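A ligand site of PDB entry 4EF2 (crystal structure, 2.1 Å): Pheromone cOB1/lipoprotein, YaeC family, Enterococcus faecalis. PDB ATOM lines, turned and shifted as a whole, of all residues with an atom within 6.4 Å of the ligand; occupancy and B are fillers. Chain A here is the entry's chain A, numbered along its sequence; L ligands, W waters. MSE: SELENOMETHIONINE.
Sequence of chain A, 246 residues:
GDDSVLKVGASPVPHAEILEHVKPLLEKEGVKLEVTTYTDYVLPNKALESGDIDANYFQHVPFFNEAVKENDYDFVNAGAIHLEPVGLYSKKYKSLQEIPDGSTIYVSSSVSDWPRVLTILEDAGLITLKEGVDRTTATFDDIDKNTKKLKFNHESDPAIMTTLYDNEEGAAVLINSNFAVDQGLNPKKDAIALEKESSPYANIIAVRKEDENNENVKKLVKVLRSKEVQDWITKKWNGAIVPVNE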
ATOM      1  N   SER A  11      16.368  -0.778   8.863  1.00  0.00           N
ATOM      2  CA  SER A  11      16.239  -2.182   8.485  1.00  0.00           C
ATOM      3  C   SER A  11      15.390  -2.917   9.535  1.00  0.00           C
ATOM      4  O   SER A  11      15.348  -2.506  10.703  1.00  0.00           O
ATOM      5  CB  SER A  11      17.618  -2.870   8.362  1.00  0.00           C
ATOM      6  OG  SER A  11      18.402  -2.266   7.314  1.00  0.00           O
ATOM      7  N   PRO A  14      18.636  -6.153  13.155  1.00  0.00           N
ATOM      8  CA  PRO A  14      18.218  -5.652  14.485  1.00  0.00           C
ATOM      9  C   PRO A  14      17.717  -4.187  14.555  1.00  0.00           C
ATOM     10  O   PRO A  14      17.168  -3.782  15.566  1.00  0.00           O
ATOM     11  CB  PRO A  14      19.534  -5.776  15.268  1.00  0.00           C
ATOM     12  CG  PRO A  14      20.578  -5.393  14.275  1.00  0.00           C
ATOM     13  CD  PRO A  14      20.099  -6.036  12.975  1.00  0.00           C
ATOM     14  N   HIS A  15      17.915  -3.374  13.506  1.00  0.00           N
ATOM     15  CA  HIS A  15      17.765  -1.920  13.643  1.00  0.00           C
ATOM     16  C   HIS A  15      16.430  -1.468  14.157  1.00  0.00           C
ATOM     17  O   HIS A  15      16.378  -0.783  15.160  1.00  0.00           O
ATOM     18  CB  HIS A  15      18.090  -1.241  12.327  1.00  0.00           C
ATOM     19  CG  HIS A  15      19.431  -1.620  11.773  1.00  0.00           C
ATOM     20  ND1 HIS A  15      19.660  -2.844  11.268  1.00  0.00           N
ATOM     21  CD2 HIS A  15      20.587  -0.885  11.551  1.00  0.00           C
ATOM     22  CE1 HIS A  15      20.908  -2.930  10.843  1.00  0.00           C
ATOM     23  NE2 HIS A  15      21.480  -1.726  10.966  1.00  0.00           N
ATOM     24  N   TYR A  41      18.252  -1.379   0.681  1.00  0.00           N
ATOM     25  CA  TYR A  41      19.339  -0.440   1.025  1.00  0.00           C
ATOM     26  C   TYR A  41      19.310   0.873   0.237  1.00  0.00           C
ATOM     27  O   TYR A  41      20.248   1.648   0.336  1.00  0.00           O
ATOM     28  CB  TYR A  41      20.710  -1.106   0.839  1.00  0.00           C
ATOM     29  CG  TYR A  41      21.125  -2.214   1.859  1.00  0.00           C
ATOM     30  CD1 TYR A  41      20.436  -2.427   3.075  1.00  0.00           C
ATOM     31  CD2 TYR A  41      22.339  -2.942   1.665  1.00  0.00           C
ATOM     32  CE1 TYR A  41      20.901  -3.383   3.993  1.00  0.00           C
ATOM     33  CE2 TYR A  41      22.793  -3.900   2.574  1.00  0.00           C
ATOM     34  CZ  TYR A  41      22.097  -4.111   3.754  1.00  0.00           C
ATOM     35  OH  TYR A  41      22.478  -5.103   4.648  1.00  0.00           O
ATOM     36  N   PHE A  58      20.641   2.008   9.257  1.00  0.00           N
ATOM     37  CA  PHE A  58      20.731   0.858   8.340  1.00  0.00           C
ATOM     38  C   PHE A  58      22.101   0.628   7.667  1.00  0.00           C
ATOM     39  O   PHE A  58      22.373  -0.492   7.304  1.00  0.00           O
ATOM     40  CB  PHE A  58      19.638   0.937   7.250  1.00  0.00           C
ATOM     41  CG  PHE A  58      20.042   1.682   6.011  1.00  0.00           C
ATOM     42  CD1 PHE A  58      20.045   3.038   5.961  1.00  0.00           C
ATOM     43  CD2 PHE A  58      20.365   0.962   4.810  1.00  0.00           C
ATOM     44  CE1 PHE A  58      20.454   3.722   4.801  1.00  0.00           C
ATOM     45  CE2 PHE A  58      20.786   1.624   3.663  1.00  0.00           C
ATOM     46  CZ  PHE A  58      20.829   3.015   3.645  1.00  0.00           C
ATOM     47  N   GLN A  59      22.930   1.667   7.499  1.00  0.00           N
ATOM     48  CA  GLN A  59      24.141   1.615   6.664  1.00  0.00           C
ATOM     49  C   GLN A  59      25.455   1.892   7.437  1.00  0.00           C
ATOM     50  O   GLN A  59      25.438   2.566   8.479  1.00  0.00           O
ATOM     51  CB  GLN A  59      24.040   2.656   5.548  1.00  0.00           C
ATOM     52  CG  GLN A  59      24.047   4.107   6.045  1.00  0.00           C
ATOM     53  CD  GLN A  59      23.666   5.151   4.992  1.00  0.00           C
ATOM     54  OE1 GLN A  59      24.060   5.038   3.849  1.00  0.00           O
ATOM     55  NE2 GLN A  59      22.909   6.192   5.393  1.00  0.00           N
ATOM     56  N   HIS A  60      26.564   1.390   6.892  1.00  0.00           N
ATOM     57  CA  HIS A  60      27.911   1.577   7.441  1.00  0.00           C
ATOM     58  C   HIS A  60      28.557   2.713   6.729  1.00  0.00           C
ATOM     59  O   HIS A  60      28.024   3.188   5.713  1.00  0.00           O
ATOM     60  CB  HIS A  60      28.789   0.299   7.507  1.00  0.00           C
ATOM     61  CG  HIS A  60      28.849  -0.534   6.225  1.00  0.00           C
ATOM     62  ND1 HIS A  60      29.292  -0.038   5.043  1.00  0.00           N
ATOM     63  CD2 HIS A  60      28.562  -1.863   6.002  1.00  0.00           C
ATOM     64  CE1 HIS A  60      29.265  -0.999   4.122  1.00  0.00           C
ATOM     65  NE2 HIS A  60      28.819  -2.113   4.691  1.00  0.00           N
ATOM     66  N   PHE A  63      29.532   2.304   2.973  1.00  0.00           N
ATOM     67  CA  PHE A  63      28.278   2.415   2.154  1.00  0.00           C
ATOM     68  C   PHE A  63      27.883   3.863   2.048  1.00  0.00           C
ATOM     69  O   PHE A  63      27.675   4.399   0.956  1.00  0.00           O
ATOM     70  CB  PHE A  63      27.138   1.522   2.804  1.00  0.00           C
ATOM     71  CG  PHE A  63      25.928   1.413   1.960  1.00  0.00           C
ATOM     72  CD1 PHE A  63      24.992   2.472   1.957  1.00  0.00           C
ATOM     73  CD2 PHE A  63      25.760   0.354   1.077  1.00  0.00           C
ATOM     74  CE1 PHE A  63      23.851   2.391   1.170  1.00  0.00           C
ATOM     75  CE2 PHE A  63      24.624   0.305   0.231  1.00  0.00           C
ATOM     76  CZ  PHE A  63      23.669   1.297   0.302  1.00  0.00           C
ATOM     77  N   PHE A  64      27.852   4.527   3.210  1.00  0.00           N
ATOM     78  CA  PHE A  64      27.384   5.912   3.330  1.00  0.00           C
ATOM     79  C   PHE A  64      28.194   6.847   2.403  1.00  0.00           C
ATOM     80  O   PHE A  64      27.615   7.719   1.732  1.00  0.00           O
ATOM     81  CB  PHE A  64      27.483   6.334   4.850  1.00  0.00           C
ATOM     82  CG  PHE A  64      27.220   7.806   5.126  1.00  0.00           C
ATOM     83  CD1 PHE A  64      25.925   8.305   5.147  1.00  0.00           C
ATOM     84  CD2 PHE A  64      28.269   8.678   5.412  1.00  0.00           C
ATOM     85  CE1 PHE A  64      25.686   9.631   5.435  1.00  0.00           C
ATOM     86  CE2 PHE A  64      28.030  10.025   5.674  1.00  0.00           C
ATOM     87  CZ  PHE A  64      26.735  10.494   5.691  1.00  0.00           C
ATOM     88  N   HIS A  82      26.589   0.149  16.060  1.00  0.00           N
ATOM     89  CA  HIS A  82      26.930  -1.320  16.213  1.00  0.00           C
ATOM     90  C   HIS A  82      27.639  -1.869  15.009  1.00  0.00           C
ATOM     91  O   HIS A  82      27.611  -1.229  13.942  1.00  0.00           O
ATOM     92  CB  HIS A  82      25.653  -2.175  16.525  1.00  0.00           C
ATOM     93  CG  HIS A  82      24.734  -2.366  15.328  1.00  0.00           C
ATOM     94  ND1 HIS A  82      23.706  -1.529  15.051  1.00  0.00           N
ATOM     95  CD2 HIS A  82      24.768  -3.303  14.295  1.00  0.00           C
ATOM     96  CE1 HIS A  82      23.123  -1.904  13.911  1.00  0.00           C
ATOM     97  NE2 HIS A  82      23.758  -3.008  13.449  1.00  0.00           N
ATOM     98  N   LEU A  83      28.218  -3.073  15.152  1.00  0.00           N
ATOM     99  CA  LEU A  83      28.887  -3.772  14.059  1.00  0.00           C
ATOM    100  C   LEU A  83      28.184  -5.104  13.750  1.00  0.00           C
ATOM    101  O   LEU A  83      27.584  -5.707  14.636  1.00  0.00           O
ATOM    102  CB  LEU A  83      30.377  -4.041  14.377  1.00  0.00           C
ATOM    103  CG  LEU A  83      31.326  -2.991  15.020  1.00  0.00           C
ATOM    104  CD1 LEU A  83      32.653  -3.639  15.393  1.00  0.00           C
ATOM    105  CD2 LEU A  83      31.617  -1.788  14.153  1.00  0.00           C
ATOM    106  N   GLU A  84      28.228  -5.535  12.486  1.00  0.00           N
ATOM    107  CA  GLU A  84      27.640  -6.842  12.044  1.00  0.00           C
ATOM    108  C   GLU A  84      28.728  -7.675  11.328  1.00  0.00           C
ATOM    109  O   GLU A  84      28.824  -7.652  10.120  1.00  0.00           O
ATOM    110  CB  GLU A  84      26.426  -6.641  11.120  1.00  0.00           C
ATOM    111  CG  GLU A  84      25.239  -5.983  11.813  1.00  0.00           C
ATOM    112  CD  GLU A  84      24.051  -5.697  10.912  1.00  0.00           C
ATOM    113  OE1 GLU A  84      23.967  -6.194   9.773  1.00  0.00           O
ATOM    114  OE2 GLU A  84      23.162  -4.976  11.358  1.00  0.00           O
ATOM    115  N   PRO A  85      29.584  -8.389  12.096  1.00  0.00           N
ATOM    116  CA  PRO A  85      30.609  -9.157  11.381  1.00  0.00           C
ATOM    117  C   PRO A  85      29.955 -10.036  10.319  1.00  0.00           C
ATOM    118  O   PRO A  85      29.082 -10.823  10.624  1.00  0.00           O
ATOM    119  CB  PRO A  85      31.268  -9.953  12.492  1.00  0.00           C
ATOM    120  CG  PRO A  85      31.089  -9.085  13.704  1.00  0.00           C
ATOM    121  CD  PRO A  85      29.738  -8.484  13.552  1.00  0.00           C
ATOM    122  N   VAL A  86      30.374  -9.847   9.085  1.00  0.00           N
ATOM    123  CA  VAL A  86      29.727 -10.514   7.924  1.00  0.00           C
ATOM    124  C   VAL A  86      30.218 -11.963   7.661  1.00  0.00           C
ATOM    125  O   VAL A  86      31.406 -12.311   7.869  1.00  0.00           O
ATOM    126  CB  VAL A  86      29.828  -9.642   6.639  1.00  0.00           C
ATOM    127  CG1 VAL A  86      31.268  -9.661   6.092  1.00  0.00           C
ATOM    128  CG2 VAL A  86      28.841 -10.150   5.613  1.00  0.00           C
ATOM    129  N   SER A 110      26.627  -4.423  -3.939  1.00  0.00           N
ATOM    130  CA  SER A 110      27.088  -3.269  -3.140  1.00  0.00           C
ATOM    131  C   SER A 110      28.625  -3.327  -3.024  1.00  0.00           C
ATOM    132  O   SER A 110      29.195  -4.102  -2.247  1.00  0.00           O
ATOM    133  CB  SER A 110      26.377  -3.290  -1.785  1.00  0.00           C
ATOM    134  OG  SER A 110      26.674  -2.118  -1.085  1.00  0.00           O
ATOM    135  N   SER A 112      30.881  -1.648  -1.633  1.00  0.00           N
ATOM    136  CA  SER A 112      31.536  -1.337  -0.347  1.00  0.00           C
ATOM    137  C   SER A 112      31.628  -2.556   0.562  1.00  0.00           C
ATOM    138  O   SER A 112      32.372  -2.529   1.554  1.00  0.00           O
ATOM    139  CB  SER A 112      30.903  -0.105   0.320  1.00  0.00           C
ATOM    140  OG  SER A 112      29.559  -0.266   0.784  1.00  0.00           O
ATOM    141  N   ASP A 113      30.907  -3.634   0.214  1.00  0.00           N
ATOM    142  CA  ASP A 113      31.079  -4.914   0.946  1.00  0.00           C
ATOM    143  C   ASP A 113      32.131  -5.833   0.307  1.00  0.00           C
ATOM    144  O   ASP A 113      32.549  -6.818   0.934  1.00  0.00           O
ATOM    145  CB  ASP A 113      29.724  -5.659   1.118  1.00  0.00           C
ATOM    146  CG  ASP A 113      28.822  -5.035   2.162  1.00  0.00           C
ATOM    147  OD1 ASP A 113      29.318  -4.569   3.202  1.00  0.00           O
ATOM    148  OD2 ASP A 113      27.573  -5.116   1.980  1.00  0.00           O
ATOM    149  N   ARG A 116      35.244  -6.990   2.216  1.00  0.00           N
ATOM    150  CA  ARG A 116      34.955  -7.829   3.357  1.00  0.00           C
ATOM    151  C   ARG A 116      35.088  -9.316   2.938  1.00  0.00           C
ATOM    152  O   ARG A 116      35.710 -10.110   3.648  1.00  0.00           O
ATOM    153  CB  ARG A 116      33.563  -7.525   3.957  1.00  0.00           C
ATOM    154  CG  ARG A 116      33.340  -6.045   4.283  1.00  0.00           C
ATOM    155  CD  ARG A 116      31.948  -5.690   4.725  1.00  0.00           C
ATOM    156  NE  ARG A 116      31.723  -6.007   6.156  1.00  0.00           N
ATOM    157  CZ  ARG A 116      30.568  -5.874   6.780  1.00  0.00           C
ATOM    158  NH1 ARG A 116      29.537  -5.429   6.139  1.00  0.00           N
ATOM    159  NH2 ARG A 116      30.418  -6.257   8.075  1.00  0.00           N
ATOM    160  N   ASN A 176      24.650 -10.021   4.329  1.00  0.00           N
ATOM    161  CA  ASN A 176      24.690  -9.031   5.437  1.00  0.00           C
ATOM    162  C   ASN A 176      23.915  -9.599   6.643  1.00  0.00           C
ATOM    163  O   ASN A 176      22.821 -10.192   6.476  1.00  0.00           O
ATOM    164  CB  ASN A 176      24.101  -7.707   5.028  1.00  0.00           C
ATOM    165  CG  ASN A 176      24.856  -7.025   3.893  1.00  0.00           C
ATOM    166  OD1 ASN A 176      24.488  -7.120   2.699  1.00  0.00           O
ATOM    167  ND2 ASN A 176      25.897  -6.315   4.257  1.00  0.00           N
ATOM    168  N   SER A 177      24.422  -9.340   7.850  1.00  0.00           N
ATOM    169  CA  SER A 177      23.804  -9.982   9.024  1.00  0.00           C
ATOM    170  C   SER A 177      22.388  -9.592   9.273  1.00  0.00           C
ATOM    171  O   SER A 177      21.588 -10.428   9.761  1.00  0.00           O
ATOM    172  CB  SER A 177      24.660  -9.804  10.275  1.00  0.00           C
ATOM    173  OG  SER A 177      25.983 -10.228  10.001  1.00  0.00           O
ATOM    174  N   ASN A 178      22.028  -8.345   8.971  1.00  0.00           N
ATOM    175  CA  ASN A 178      20.644  -7.913   9.137  1.00  0.00           C
ATOM    176  C   ASN A 178      19.665  -8.806   8.353  1.00  0.00           C
ATOM    177  O   ASN A 178      18.612  -9.194   8.847  1.00  0.00           O
ATOM    178  CB  ASN A 178      20.459  -6.407   8.802  1.00  0.00           C
ATOM    179  CG  ASN A 178      20.480  -6.113   7.318  1.00  0.00           C
ATOM    180  OD1 ASN A 178      21.531  -6.070   6.733  1.00  0.00           O
ATOM    181  ND2 ASN A 178      19.295  -5.861   6.722  1.00  0.00           N
ATOM    182  N   TYR A 201      33.043  -1.133   9.591  1.00  0.00           N
ATOM    183  CA  TYR A 201      31.677  -1.323   9.133  1.00  0.00           C
ATOM    184  C   TYR A 201      30.608  -1.095  10.206  1.00  0.00           C
ATOM    185  O   TYR A 201      29.568  -1.741  10.191  1.00  0.00           O
ATOM    186  CB  TYR A 201      31.547  -2.717   8.453  1.00  0.00           C
ATOM    187  CG  TYR A 201      32.521  -2.861   7.335  1.00  0.00           C
ATOM    188  CD1 TYR A 201      32.298  -2.218   6.097  1.00  0.00           C
ATOM    189  CD2 TYR A 201      33.754  -3.552   7.530  1.00  0.00           C
ATOM    190  CE1 TYR A 201      33.216  -2.314   5.064  1.00  0.00           C
ATOM    191  CE2 TYR A 201      34.671  -3.654   6.489  1.00  0.00           C
ATOM    192  CZ  TYR A 201      34.419  -2.998   5.271  1.00  0.00           C
ATOM    193  OH  TYR A 201      35.304  -3.043   4.218  1.00  0.00           O
ATOM    194  N   ALA A 202      30.883  -0.157  11.109  1.00  0.00           N
ATOM    195  CA  ALA A 202      29.955   0.317  12.114  1.00  0.00           C
ATOM    196  C   ALA A 202      28.718   0.930  11.446  1.00  0.00           C
ATOM    197  O   ALA A 202      28.803   1.787  10.517  1.00  0.00           O
ATOM    198  CB  ALA A 202      30.658   1.366  13.025  1.00  0.00           C
ATOM    199  N   ASN A 203      27.554   0.437  11.845  1.00  0.00           N
ATOM    200  CA  ASN A 203      26.286   0.974  11.357  1.00  0.00           C
ATOM    201  C   ASN A 203      25.990   2.282  12.095  1.00  0.00           C
ATOM    202  O   ASN A 203      26.111   2.344  13.323  1.00  0.00           O
ATOM    203  CB  ASN A 203      25.155  -0.051  11.521  1.00  0.00           C
ATOM    204  CG  ASN A 203      25.216  -1.188  10.500  1.00  0.00           C
ATOM    205  OD1 ASN A 203      24.191  -1.628  10.032  1.00  0.00           O
ATOM    206  ND2 ASN A 203      26.425  -1.684  10.157  1.00  0.00           N
HETATM  207  N   MSE L   1      23.659  -3.981   8.373  1.00  0.00           N
HETATM  208  CA  MSE L   1      24.557  -4.073   7.229  1.00  0.00           C
HETATM  209  C   MSE L   1      25.992  -4.549   7.626  1.00  0.00           C
HETATM  210  O   MSE L   1      26.517  -4.048   8.589  1.00  0.00           O
HETATM  211  OXT MSE L   1      26.638  -5.394   6.957  1.00  0.00           O
HETATM  212  CB  MSE L   1      24.639  -2.713   6.442  1.00  0.00           C
HETATM  213  CG  MSE L   1      25.273  -2.873   5.052  1.00  0.00           C
HETATM  214 SE   MSE L   1      25.581  -1.040   4.209  1.00  0.00          SE
HETATM  215  CE  MSE L   1      23.710  -0.530   3.729  1.00  0.00           C
HETATM  216  O   HOH W   1      26.023  -3.011   1.396  1.00  0.00           O
HETATM  217  O   HOH W   2      28.849  -4.345   9.912  1.00  0.00           O
HETATM  218  O   HOH W   3      21.153  -2.939   7.526  1.00  0.00           O
HETATM  219  O   HOH W   4      27.035  -7.981   7.856  1.00  0.00           O
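The backbone NH of Asn 178 is in hydrogen-bond range of the side-chain carboxylate of Glu 84, 3.0 Å away.
The side-chain carboxylate (OE2) of Glu 84 lies within hydrogen-bond range of a ring nitrogen (NE2) of His 82 (2.9 Å).
The side-chain amide oxygen (OD1) of Asn 203 sits close to the backbone carbonyl oxygen (O) of Phe 58, at 3.5 Å.
A ring nitrogen (NE2) of His 15 is in hydrogen-bond range of the side-chain amide oxygen (OD1) of Asn 203 (2.9 Å).
ND2 of Asn 203 lies within hydrogen-bond range of O of Tyr 201, 3.1 Å away.
The backbone NH (N) of Asn 203 is in hydrogen-bond range of the backbone carbonyl oxygen (O) of His 82 (2.7 Å).
ND2 of Asn 176 lies within hydrogen-bond range of OD2 of Asp 113 (3.1 Å).
The backbone NH (N) of Phe 63 lies close to the side-chain hydroxyl (OG) of Ser 112 (3.4 Å).
Water W2 lies within hydrogen-bond range of O of the ligand (2.7 Å), O of Tyr 201 (2.7 Å), N of Glu 84 (2.9 Å) and NH2 of Arg 116 (3.1 Å).
Water W4 lies within hydrogen-bond range of OXT of the ligand (2.8 Å), O of Glu 84 (2.9 Å) and N of Ser 177 (2.9 Å).
Water W3 lies within hydrogen-bond range of O of Phe 58 (2.7 Å), OG of Ser 11 (2.8 Å), N of the ligand (2.8 Å) and OD1 of Asn 178 (3.3 Å).
Water W1 bridges OD2 of Asp 113 (2.7 Å) and OG of Ser 110 (2.7 Å).
His 15 touches the ligand (CE1 to N, 3.8 Å).
Tyr 41 touches the ligand.
Phe 58 touches the ligand.
Gln 59 touches the ligand (CA to CE, 3.7 Å).
NE2 of His 60 touches SE of the ligand (3.4 Å).
CB of Phe 63 touches SE of the ligand, at 3.3 Å.
Hydrophobic or aromatic side chains that line the ligand: His 15, Tyr 41, Phe 58, His 60 and Phe 63.
Along chain A the residues within 4 Å of the ligand span positions 15 to 203.
A nitrogen (N) of the ligand lies within salt-bridge range of the side-chain carboxylate (OE1) of Glu 84 (2.6 Å).
ND2 of Asn 203 sits at hydrogen-bond distance from O of the ligand (2.8 Å).
The side-chain amide nitrogen (ND2) of Asn 176 is in hydrogen-bond range of an oxygen (OXT) of the ligand, 2.9 Å away.
An oxygen (OXT) of the ligand lies within salt-bridge range of the guanidinium group (NH1) of Arg 116, 3.0 Å away.
N of the ligand lies within hydrogen-bond range of OD1 of Asn 178 (3.4 Å).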
